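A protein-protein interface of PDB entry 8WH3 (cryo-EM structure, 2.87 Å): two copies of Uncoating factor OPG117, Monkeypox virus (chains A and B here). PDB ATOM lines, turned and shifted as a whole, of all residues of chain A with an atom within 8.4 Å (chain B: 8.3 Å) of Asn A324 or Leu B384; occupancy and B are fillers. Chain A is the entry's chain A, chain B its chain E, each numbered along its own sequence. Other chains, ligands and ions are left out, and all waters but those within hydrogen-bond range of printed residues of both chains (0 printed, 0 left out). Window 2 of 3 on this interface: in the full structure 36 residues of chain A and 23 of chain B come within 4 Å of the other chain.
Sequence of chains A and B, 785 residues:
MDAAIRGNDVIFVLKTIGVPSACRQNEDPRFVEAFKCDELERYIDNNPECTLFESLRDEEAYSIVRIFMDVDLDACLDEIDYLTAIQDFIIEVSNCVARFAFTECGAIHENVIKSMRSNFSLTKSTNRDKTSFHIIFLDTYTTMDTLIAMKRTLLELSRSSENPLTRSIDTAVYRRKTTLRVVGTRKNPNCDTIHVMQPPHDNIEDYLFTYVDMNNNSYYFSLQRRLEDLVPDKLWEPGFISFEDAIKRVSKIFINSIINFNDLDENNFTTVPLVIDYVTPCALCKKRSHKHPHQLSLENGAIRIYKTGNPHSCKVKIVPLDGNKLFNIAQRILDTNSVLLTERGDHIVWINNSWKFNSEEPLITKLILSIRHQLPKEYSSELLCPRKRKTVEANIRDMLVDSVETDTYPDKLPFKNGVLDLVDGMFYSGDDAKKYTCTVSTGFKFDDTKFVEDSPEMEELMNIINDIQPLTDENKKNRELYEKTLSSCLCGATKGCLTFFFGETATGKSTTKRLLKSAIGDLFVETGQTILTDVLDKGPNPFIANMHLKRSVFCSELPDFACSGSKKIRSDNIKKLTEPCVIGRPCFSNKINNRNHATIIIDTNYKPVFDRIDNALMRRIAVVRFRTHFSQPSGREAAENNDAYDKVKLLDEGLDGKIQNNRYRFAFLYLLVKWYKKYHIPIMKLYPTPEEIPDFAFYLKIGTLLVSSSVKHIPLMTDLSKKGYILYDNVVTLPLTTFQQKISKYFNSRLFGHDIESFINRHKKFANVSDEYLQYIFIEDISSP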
ATOM      1  N   GLY A 323       9.505  26.074   0.223  1.00  0.00           N
ATOM      2  CA  GLY A 323       9.311  25.497   1.540  1.00  0.00           C
ATOM      3  C   GLY A 323       9.555  24.002   1.579  1.00  0.00           C
ATOM      4  O   GLY A 323       8.771  23.225   1.034  1.00  0.00           O
ATOM      5  N   ASN A 324      10.646  23.606   2.236  1.00  0.00           N
ATOM      6  CA  ASN A 324      11.027  22.203   2.348  1.00  0.00           C
ATOM      7  C   ASN A 324      11.219  21.557   0.984  1.00  0.00           C
ATOM      8  O   ASN A 324      10.408  20.727   0.566  1.00  0.00           O
ATOM      9  CB  ASN A 324      10.010  21.419   3.174  1.00  0.00           C
ATOM     10  CG  ASN A 324      10.520  21.104   4.560  1.00  0.00           C
ATOM     11  OD1 ASN A 324      11.253  20.137   4.756  1.00  0.00           O
ATOM     12  ND2 ASN A 324      10.141  21.924   5.533  1.00  0.00           N
ATOM     13  N   LYS A 325      12.267  21.975   0.270  1.00  0.00           N
ATOM     14  CA  LYS A 325      12.626  21.331  -0.989  1.00  0.00           C
ATOM     15  C   LYS A 325      12.739  19.821  -0.833  1.00  0.00           C
ATOM     16  O   LYS A 325      12.317  19.065  -1.715  1.00  0.00           O
ATOM     17  CB  LYS A 325      13.949  21.898  -1.503  1.00  0.00           C
ATOM     18  CG  LYS A 325      13.824  23.178  -2.295  1.00  0.00           C
ATOM     19  CD  LYS A 325      15.192  23.736  -2.627  1.00  0.00           C
ATOM     20  CE  LYS A 325      15.706  23.176  -3.937  1.00  0.00           C
ATOM     21  NZ  LYS A 325      14.854  23.597  -5.080  1.00  0.00           N
ATOM     22  N   LEU A 326      13.311  19.360   0.281  1.00  0.00           N
ATOM     23  CA  LEU A 326      13.521  17.929   0.466  1.00  0.00           C
ATOM     24  C   LEU A 326      12.205  17.178   0.623  1.00  0.00           C
ATOM     25  O   LEU A 326      12.074  16.051   0.131  1.00  0.00           O
ATOM     26  CB  LEU A 326      14.433  17.691   1.668  1.00  0.00           C
ATOM     27  CG  LEU A 326      15.812  18.353   1.580  1.00  0.00           C
ATOM     28  CD1 LEU A 326      16.670  17.986   2.770  1.00  0.00           C
ATOM     29  CD2 LEU A 326      16.521  17.996   0.286  1.00  0.00           C
ATOM     30  N   PHE A 327      11.215  17.785   1.281  1.00  0.00           N
ATOM     31  CA  PHE A 327       9.910  17.145   1.401  1.00  0.00           C
ATOM     32  C   PHE A 327       9.209  17.061   0.051  1.00  0.00           C
ATOM     33  O   PHE A 327       8.556  16.058  -0.253  1.00  0.00           O
ATOM     34  CB  PHE A 327       9.045  17.894   2.411  1.00  0.00           C
ATOM     35  CG  PHE A 327       7.787  17.169   2.782  1.00  0.00           C
ATOM     36  CD1 PHE A 327       7.799  16.192   3.759  1.00  0.00           C
ATOM     37  CD2 PHE A 327       6.592  17.459   2.152  1.00  0.00           C
ATOM     38  CE1 PHE A 327       6.647  15.524   4.103  1.00  0.00           C
ATOM     39  CE2 PHE A 327       5.438  16.788   2.489  1.00  0.00           C
ATOM     40  CZ  PHE A 327       5.467  15.821   3.466  1.00  0.00           C
ATOM     41  N   ASN A 328       9.333  18.101  -0.774  1.00  0.00           N
ATOM     42  CA  ASN A 328       8.763  18.049  -2.117  1.00  0.00           C
ATOM     43  C   ASN A 328       9.458  16.997  -2.974  1.00  0.00           C
ATOM     44  O   ASN A 328       8.809  16.310  -3.772  1.00  0.00           O
ATOM     45  CB  ASN A 328       8.850  19.423  -2.773  1.00  0.00           C
ATOM     46  CG  ASN A 328       8.094  20.483  -2.000  1.00  0.00           C
ATOM     47  OD1 ASN A 328       7.201  20.174  -1.214  1.00  0.00           O
ATOM     48  ND2 ASN A 328       8.448  21.742  -2.222  1.00  0.00           N
ATOM     49  N   ILE A 329      10.778  16.863  -2.829  1.00  0.00           N
ATOM     50  CA  ILE A 329      11.507  15.815  -3.540  1.00  0.00           C
ATOM     51  C   ILE A 329      10.996  14.443  -3.123  1.00  0.00           C
ATOM     52  O   ILE A 329      10.774  13.559  -3.959  1.00  0.00           O
ATOM     53  CB  ILE A 329      13.019  15.951  -3.289  1.00  0.00           C
ATOM     54  CG1 ILE A 329      13.561  17.216  -3.947  1.00  0.00           C
ATOM     55  CG2 ILE A 329      13.756  14.741  -3.811  1.00  0.00           C
ATOM     56  CD1 ILE A 329      14.980  17.526  -3.568  1.00  0.00           C
ATOM     57  N   ALA A 330      10.808  14.246  -1.818  1.00  0.00           N
ATOM     58  CA  ALA A 330      10.283  12.976  -1.329  1.00  0.00           C
ATOM     59  C   ALA A 330       8.878  12.719  -1.855  1.00  0.00           C
ATOM     60  O   ALA A 330       8.533  11.580  -2.195  1.00  0.00           O
ATOM     61  CB  ALA A 330      10.301  12.960   0.196  1.00  0.00           C
ATOM     62  N   GLN A 331       8.051  13.764  -1.930  1.00  0.00           N
ATOM     63  CA  GLN A 331       6.700  13.611  -2.464  1.00  0.00           C
ATOM     64  C   GLN A 331       6.725  13.202  -3.931  1.00  0.00           C
ATOM     65  O   GLN A 331       5.952  12.337  -4.354  1.00  0.00           O
ATOM     66  CB  GLN A 331       5.914  14.907  -2.287  1.00  0.00           C
ATOM     67  CG  GLN A 331       4.937  14.891  -1.131  1.00  0.00           C
ATOM     68  CD  GLN A 331       3.687  14.100  -1.441  1.00  0.00           C
ATOM     69  OE1 GLN A 331       3.184  14.130  -2.562  1.00  0.00           O
ATOM     70  NE2 GLN A 331       3.174  13.387  -0.447  1.00  0.00           N
ATOM     71  N   TYR A 379      15.903  20.601  -8.222  1.00  0.00           N
ATOM     72  CA  TYR A 379      15.831  19.463  -7.320  1.00  0.00           C
ATOM     73  C   TYR A 379      16.964  18.469  -7.521  1.00  0.00           C
ATOM     74  O   TYR A 379      17.252  17.690  -6.608  1.00  0.00           O
ATOM     75  CB  TYR A 379      14.495  18.732  -7.490  1.00  0.00           C
ATOM     76  CG  TYR A 379      13.307  19.459  -6.903  1.00  0.00           C
ATOM     77  CD1 TYR A 379      13.465  20.656  -6.222  1.00  0.00           C
ATOM     78  CD2 TYR A 379      12.026  18.943  -7.027  1.00  0.00           C
ATOM     79  CE1 TYR A 379      12.383  21.319  -5.685  1.00  0.00           C
ATOM     80  CE2 TYR A 379      10.939  19.599  -6.493  1.00  0.00           C
ATOM     81  CZ  TYR A 379      11.125  20.786  -5.824  1.00  0.00           C
ATOM     82  OH  TYR A 379      10.043  21.443  -5.289  1.00  0.00           O
ATOM     83  N   GLU A 382      20.360  19.062  -5.321  1.00  0.00           N
ATOM     84  CA  GLU A 382      20.284  18.797  -3.892  1.00  0.00           C
ATOM     85  C   GLU A 382      20.467  17.327  -3.553  1.00  0.00           C
ATOM     86  O   GLU A 382      20.538  16.985  -2.371  1.00  0.00           O
ATOM     87  CB  GLU A 382      18.945  19.280  -3.330  1.00  0.00           C
ATOM     88  CG  GLU A 382      18.739  20.777  -3.410  1.00  0.00           C
ATOM     89  CD  GLU A 382      19.236  21.503  -2.176  1.00  0.00           C
ATOM     90  OE1 GLU A 382      18.633  21.327  -1.096  1.00  0.00           O
ATOM     91  OE2 GLU A 382      20.228  22.252  -2.285  1.00  0.00           O
ATOM     92  N   THR A 391      18.003  12.615   4.526  1.00  0.00           N
ATOM     93  CA  THR A 391      16.778  13.304   4.929  1.00  0.00           C
ATOM     94  C   THR A 391      15.602  12.921   4.035  1.00  0.00           C
ATOM     95  O   THR A 391      14.486  12.688   4.522  1.00  0.00           O
ATOM     96  CB  THR A 391      16.992  14.816   4.907  1.00  0.00           C
ATOM     97  OG1 THR A 391      18.036  15.165   5.820  1.00  0.00           O
ATOM     98  CG2 THR A 391      15.725  15.536   5.310  1.00  0.00           C
ATOM     99  N   ALA A 394      14.421   9.515   5.022  1.00  0.00           N
ATOM    100  CA  ALA A 394      13.624   9.560   6.247  1.00  0.00           C
ATOM    101  C   ALA A 394      12.201  10.025   5.966  1.00  0.00           C
ATOM    102  O   ALA A 394      11.232   9.452   6.485  1.00  0.00           O
ATOM    103  CB  ALA A 394      14.291  10.473   7.272  1.00  0.00           C
ATOM    104  N   ASN A 395      12.056  11.060   5.137  1.00  0.00           N
ATOM    105  CA  ASN A 395      10.724  11.521   4.751  1.00  0.00           C
ATOM    106  C   ASN A 395       9.944  10.414   4.050  1.00  0.00           C
ATOM    107  O   ASN A 395       8.762  10.192   4.335  1.00  0.00           O
ATOM    108  CB  ASN A 395      10.839  12.747   3.849  1.00  0.00           C
ATOM    109  CG  ASN A 395      10.972  14.032   4.627  1.00  0.00           C
ATOM    110  OD1 ASN A 395      10.266  14.252   5.603  1.00  0.00           O
ATOM    111  ND2 ASN A 395      11.878  14.893   4.193  1.00  0.00           N
ATOM    112  N   ASP A 398       8.741   7.784   6.500  1.00  0.00           N
ATOM    113  CA  ASP A 398       7.577   8.226   7.264  1.00  0.00           C
ATOM    114  C   ASP A 398       6.316   8.261   6.409  1.00  0.00           C
ATOM    115  O   ASP A 398       5.215   8.058   6.929  1.00  0.00           O
ATOM    116  CB  ASP A 398       7.829   9.601   7.874  1.00  0.00           C
ATOM    117  CG  ASP A 398       8.672   9.534   9.123  1.00  0.00           C
ATOM    118  OD1 ASP A 398       8.876   8.419   9.641  1.00  0.00           O
ATOM    119  OD2 ASP A 398       9.135  10.595   9.587  1.00  0.00           O
ATOM    120  N   MET A 399       6.450   8.524   5.107  1.00  0.00           N
ATOM    121  CA  MET A 399       5.276   8.662   4.252  1.00  0.00           C
ATOM    122  C   MET A 399       4.608   7.334   3.922  1.00  0.00           C
ATOM    123  O   MET A 399       3.422   7.326   3.579  1.00  0.00           O
ATOM    124  CB  MET A 399       5.651   9.367   2.953  1.00  0.00           C
ATOM    125  CG  MET A 399       5.745  10.869   3.064  1.00  0.00           C
ATOM    126  SD  MET A 399       5.995  11.623   1.453  1.00  0.00           S
ATOM    127  CE  MET A 399       7.137  12.921   1.877  1.00  0.00           C
ATOM    128  N   ILE B 368       2.773  11.514  13.614  1.00  0.00           N
ATOM    129  CA  ILE B 368       2.984  12.959  13.619  1.00  0.00           C
ATOM    130  C   ILE B 368       2.807  13.521  12.215  1.00  0.00           C
ATOM    131  O   ILE B 368       2.097  14.515  12.004  1.00  0.00           O
ATOM    132  CB  ILE B 368       4.372  13.300  14.191  1.00  0.00           C
ATOM    133  CG1 ILE B 368       4.451  12.927  15.667  1.00  0.00           C
ATOM    134  CG2 ILE B 368       4.673  14.771  14.018  1.00  0.00           C
ATOM    135  CD1 ILE B 368       5.849  12.706  16.156  1.00  0.00           C
ATOM    136  N   LEU B 369       3.430  12.875  11.228  1.00  0.00           N
ATOM    137  CA  LEU B 369       3.315  13.344   9.852  1.00  0.00           C
ATOM    138  C   LEU B 369       1.873  13.286   9.363  1.00  0.00           C
ATOM    139  O   LEU B 369       1.410  14.198   8.671  1.00  0.00           O
ATOM    140  CB  LEU B 369       4.228  12.524   8.942  1.00  0.00           C
ATOM    141  CG  LEU B 369       4.478  13.076   7.539  1.00  0.00           C
ATOM    142  CD1 LEU B 369       4.995  14.496   7.602  1.00  0.00           C
ATOM    143  CD2 LEU B 369       5.443  12.192   6.788  1.00  0.00           C
ATOM    144  N   ARG B 372      -0.344  16.008  11.155  1.00  0.00           N
ATOM    145  CA  ARG B 372       0.036  17.397  10.912  1.00  0.00           C
ATOM    146  C   ARG B 372      -1.074  18.240  10.292  1.00  0.00           C
ATOM    147  O   ARG B 372      -1.016  19.471  10.373  1.00  0.00           O
ATOM    148  CB  ARG B 372       1.273  17.442  10.013  1.00  0.00           C
ATOM    149  CG  ARG B 372       0.981  17.689   8.547  1.00  0.00           C
ATOM    150  CD  ARG B 372       2.257  17.685   7.733  1.00  0.00           C
ATOM    151  NE  ARG B 372       1.991  17.698   6.300  1.00  0.00           N
ATOM    152  CZ  ARG B 372       1.760  16.615   5.572  1.00  0.00           C
ATOM    153  NH1 ARG B 372       1.738  15.410   6.115  1.00  0.00           N
ATOM    154  NH2 ARG B 372       1.546  16.745   4.267  1.00  0.00           N
ATOM    155  N   HIS B 373      -2.081  17.617   9.676  1.00  0.00           N
ATOM    156  CA  HIS B 373      -3.133  18.382   9.014  1.00  0.00           C
ATOM    157  C   HIS B 373      -4.134  18.980   9.997  1.00  0.00           C
ATOM    158  O   HIS B 373      -4.625  20.090   9.768  1.00  0.00           O
ATOM    159  CB  HIS B 373      -3.862  17.502   8.001  1.00  0.00           C
ATOM    160  CG  HIS B 373      -3.113  17.315   6.720  1.00  0.00           C
ATOM    161  ND1 HIS B 373      -2.611  18.371   5.991  1.00  0.00           N
ATOM    162  CD2 HIS B 373      -2.778  16.194   6.039  1.00  0.00           C
ATOM    163  CE1 HIS B 373      -2.002  17.910   4.914  1.00  0.00           C
ATOM    164  NE2 HIS B 373      -2.089  16.592   4.919  1.00  0.00           N
ATOM    165  N   TYR B 379       1.729  25.477  12.956  1.00  0.00           N
ATOM    166  CA  TYR B 379       2.292  24.262  13.527  1.00  0.00           C
ATOM    167  C   TYR B 379       2.552  23.176  12.497  1.00  0.00           C
ATOM    168  O   TYR B 379       3.354  22.276  12.755  1.00  0.00           O
ATOM    169  CB  TYR B 379       1.359  23.700  14.605  1.00  0.00           C
ATOM    170  CG  TYR B 379       1.375  24.463  15.907  1.00  0.00           C
ATOM    171  CD1 TYR B 379       2.196  25.567  16.079  1.00  0.00           C
ATOM    172  CD2 TYR B 379       0.574  24.072  16.967  1.00  0.00           C
ATOM    173  CE1 TYR B 379       2.215  26.262  17.268  1.00  0.00           C
ATOM    174  CE2 TYR B 379       0.585  24.761  18.158  1.00  0.00           C
ATOM    175  CZ  TYR B 379       1.408  25.854  18.304  1.00  0.00           C
ATOM    176  OH  TYR B 379       1.423  26.544  19.493  1.00  0.00           O
ATOM    177  N   SER B 380       1.891  23.239  11.340  1.00  0.00           N
ATOM    178  CA  SER B 380       2.018  22.176  10.350  1.00  0.00           C
ATOM    179  C   SER B 380       3.335  22.253   9.589  1.00  0.00           C
ATOM    180  O   SER B 380       3.850  21.223   9.143  1.00  0.00           O
ATOM    181  CB  SER B 380       0.843  22.230   9.377  1.00  0.00           C
ATOM    182  OG  SER B 380      -0.324  21.684   9.963  1.00  0.00           O
ATOM    183  N   SER B 381       3.889  23.454   9.423  1.00  0.00           N
ATOM    184  CA  SER B 381       5.119  23.593   8.651  1.00  0.00           C
ATOM    185  C   SER B 381       6.322  23.024   9.391  1.00  0.00           C
ATOM    186  O   SER B 381       7.312  22.645   8.756  1.00  0.00           O
ATOM    187  CB  SER B 381       5.358  25.062   8.308  1.00  0.00           C
ATOM    188  OG  SER B 381       5.074  25.895   9.418  1.00  0.00           O
ATOM    189  N   GLU B 382       6.263  22.963  10.721  1.00  0.00           N
ATOM    190  CA  GLU B 382       7.378  22.448  11.507  1.00  0.00           C
ATOM    191  C   GLU B 382       7.454  20.929  11.503  1.00  0.00           C
ATOM    192  O   GLU B 382       8.470  20.378  11.933  1.00  0.00           O
ATOM    193  CB  GLU B 382       7.278  22.951  12.945  1.00  0.00           C
ATOM    194  CG  GLU B 382       7.304  24.457  13.065  1.00  0.00           C
ATOM    195  CD  GLU B 382       8.709  25.016  13.009  1.00  0.00           C
ATOM    196  OE1 GLU B 382       9.474  24.805  13.973  1.00  0.00           O
ATOM    197  OE2 GLU B 382       9.053  25.664  11.998  1.00  0.00           O
ATOM    198  N   LEU B 383       6.418  20.245  11.033  1.00  0.00           N
ATOM    199  CA  LEU B 383       6.361  18.794  11.067  1.00  0.00           C
ATOM    200  C   LEU B 383       6.838  18.157   9.771  1.00  0.00           C
ATOM    201  O   LEU B 383       6.669  16.948   9.591  1.00  0.00           O
ATOM    202  CB  LEU B 383       4.940  18.336  11.390  1.00  0.00           C
ATOM    203  CG  LEU B 383       4.433  18.800  12.754  1.00  0.00           C
ATOM    204  CD1 LEU B 383       3.071  18.215  13.046  1.00  0.00           C
ATOM    205  CD2 LEU B 383       5.424  18.420  13.840  1.00  0.00           C
ATOM    206  N   LEU B 384       7.421  18.938   8.867  1.00  0.00           N
ATOM    207  CA  LEU B 384       7.977  18.422   7.626  1.00  0.00           C
ATOM    208  C   LEU B 384       9.466  18.113   7.722  1.00  0.00           C
ATOM    209  O   LEU B 384      10.066  17.717   6.719  1.00  0.00           O
ATOM    210  CB  LEU B 384       7.734  19.414   6.488  1.00  0.00           C
ATOM    211  CG  LEU B 384       6.284  19.787   6.195  1.00  0.00           C
ATOM    212  CD1 LEU B 384       6.205  20.678   4.978  1.00  0.00           C
ATOM    213  CD2 LEU B 384       5.455  18.542   5.994  1.00  0.00           C
ATOM    214  N   CYS B 385      10.075  18.283   8.896  1.00  0.00           N
ATOM    215  CA  CYS B 385      11.485  17.991   9.113  1.00  0.00           C
ATOM    216  C   CYS B 385      11.629  16.760   9.991  1.00  0.00           C
ATOM    217  O   CYS B 385      10.961  16.674  11.029  1.00  0.00           O
ATOM    218  CB  CYS B 385      12.183  19.180   9.768  1.00  0.00           C
ATOM    219  SG  CYS B 385      13.988  19.097   9.782  1.00  0.00           S
ATOM    220  N   PRO B 386      12.452  15.782   9.609  1.00  0.00           N
ATOM    221  CA  PRO B 386      12.616  14.592  10.460  1.00  0.00           C
ATOM    222  C   PRO B 386      13.171  14.888  11.844  1.00  0.00           C
ATOM    223  O   PRO B 386      12.788  14.213  12.807  1.00  0.00           O
ATOM    224  CB  PRO B 386      13.571  13.714   9.641  1.00  0.00           C
ATOM    225  CG  PRO B 386      13.413  14.175   8.246  1.00  0.00           C
ATOM    226  CD  PRO B 386      13.151  15.639   8.323  1.00  0.00           C
ATOM    227  N   ARG B 387      14.066  15.870  11.974  1.00  0.00           N
ATOM    228  CA  ARG B 387      14.613  16.210  13.285  1.00  0.00           C
ATOM    229  C   ARG B 387      13.532  16.733  14.222  1.00  0.00           C
ATOM    230  O   ARG B 387      13.470  16.345  15.396  1.00  0.00           O
ATOM    231  CB  ARG B 387      15.714  17.252  13.138  1.00  0.00           C
ATOM    232  CG  ARG B 387      17.039  16.730  12.638  1.00  0.00           C
ATOM    233  CD  ARG B 387      18.144  17.781  12.773  1.00  0.00           C
ATOM    234  NE  ARG B 387      17.793  19.065  12.175  1.00  0.00           N
ATOM    235  CZ  ARG B 387      17.281  20.095  12.836  1.00  0.00           C
ATOM    236  NH1 ARG B 387      17.064  20.043  14.140  1.00  0.00           N
ATOM    237  NH2 ARG B 387      16.978  21.208  12.172  1.00  0.00           N
ATOM    238  N   LYS B 388      12.682  17.628  13.724  1.00  0.00           N
ATOM    239  CA  LYS B 388      11.627  18.187  14.556  1.00  0.00           C
ATOM    240  C   LYS B 388      10.599  17.127  14.922  1.00  0.00           C
ATOM    241  O   LYS B 388      10.070  17.124  16.040  1.00  0.00           O
ATOM    242  CB  LYS B 388      10.980  19.362  13.835  1.00  0.00           C
ATOM    243  CG  LYS B 388      11.922  20.533  13.643  1.00  0.00           C
ATOM    244  CD  LYS B 388      11.249  21.671  12.907  1.00  0.00           C
ATOM    245  CE  LYS B 388      12.060  22.949  12.989  1.00  0.00           C
ATOM    246  NZ  LYS B 388      13.209  22.818  13.917  1.00  0.00           N
ATOM    247  N   ARG B 389      10.313  16.209  13.999  1.00  0.00           N
ATOM    248  CA  ARG B 389       9.414  15.107  14.314  1.00  0.00           C
ATOM    249  C   ARG B 389      10.011  14.204  15.384  1.00  0.00           C
ATOM    250  O   ARG B 389       9.291  13.699  16.251  1.00  0.00           O
ATOM    251  CB  ARG B 389       9.090  14.315  13.050  1.00  0.00           C
ATOM    252  CG  ARG B 389       8.264  15.089  12.040  1.00  0.00           C
ATOM    253  CD  ARG B 389       7.511  14.172  11.096  1.00  0.00           C
ATOM    254  NE  ARG B 389       8.397  13.332  10.301  1.00  0.00           N
ATOM    255  CZ  ARG B 389       8.814  13.624   9.078  1.00  0.00           C
ATOM    256  NH1 ARG B 389       8.463  14.747   8.478  1.00  0.00           N
ATOM    257  NH2 ARG B 389       9.600  12.766   8.438  1.00  0.00           N
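The side-chain amide oxygen (OD1) of Asn A395 is in hydrogen-bond range of the guanidinium group (NH2) of Arg B389, at 3.3 Å.
NH2 of Arg B389 is in salt-bridge range of OD2 of Asp A398 (2.5 Å).
O of Leu B384 sits close to OD1 of Asn A324 (3.3 Å).
The backbone carbonyl oxygen (O) of Leu B383 lies within hydrogen-bond range of the guanidinium group (NH1) of Arg B389 (3.0 Å).
NH1 of Arg B372 sits at hydrogen-bond distance from O of Leu B369 (2.8 Å).
ND2 of Asn A395 sits at hydrogen-bond distance from O of Thr A391 (3.4 Å).
No residue of chain B comes within 4 Å of Gly A323.
Printed residues of chain B within 4 Å of Thr A391: Pro B386.
Printed residues of chain B within 4 Å of Asp A398: Leu B369 (3.7 Å) and Arg B389 (2.5 Å).
Of the printed residues of chain B, Met A399 touches Leu B369 (3.96 Å).
Of the printed residues of chain A, Leu B369 touches Asp A398 and Met A399.
Ser B380 touches none of the printed residues of chain A.
Leu B384 touches just these residues of chain A: Asn A324, Phe A327 and Asn A395.
The nearest residue of chain A that does not touch Leu B384 is Gly A323 (5.4 Å).
The nearest printed residue of chain B that does not touch Asn A395 is Pro B386 (4.1 Å).
Of the 15 printed residues of chain B, 4 touch a printed residue of chain A.
Hydrophobic or aromatic side chains of chain B within 4 Å of the printed part of chain A: Leu B369, Leu B384 and Pro B386.
Hydrophobic or aromatic side chains of chain A within 4 Å of the printed part of chain B: Phe A327, Ala A394 and Met A399.
Among the printed residues, Asp or Glu carboxylates within 4 Å of a Lys or Arg side-chain nitrogen of the other chain: Asp A398 with Arg B389 (2.5 Å).
2 positions are printed for both chains.
Of the 9 pairs that touch across the chains among the printed residues, none has its exchanged pair printed and touching as well.
Among the printed residues, merely in contact across the chains: Asn A395 with Leu B384, Asp A398 with Leu B369, Phe A327 with Leu B384, Ala A394 with Pro B386, Met A399 with Leu B369 and Thr A391 with Pro B386.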
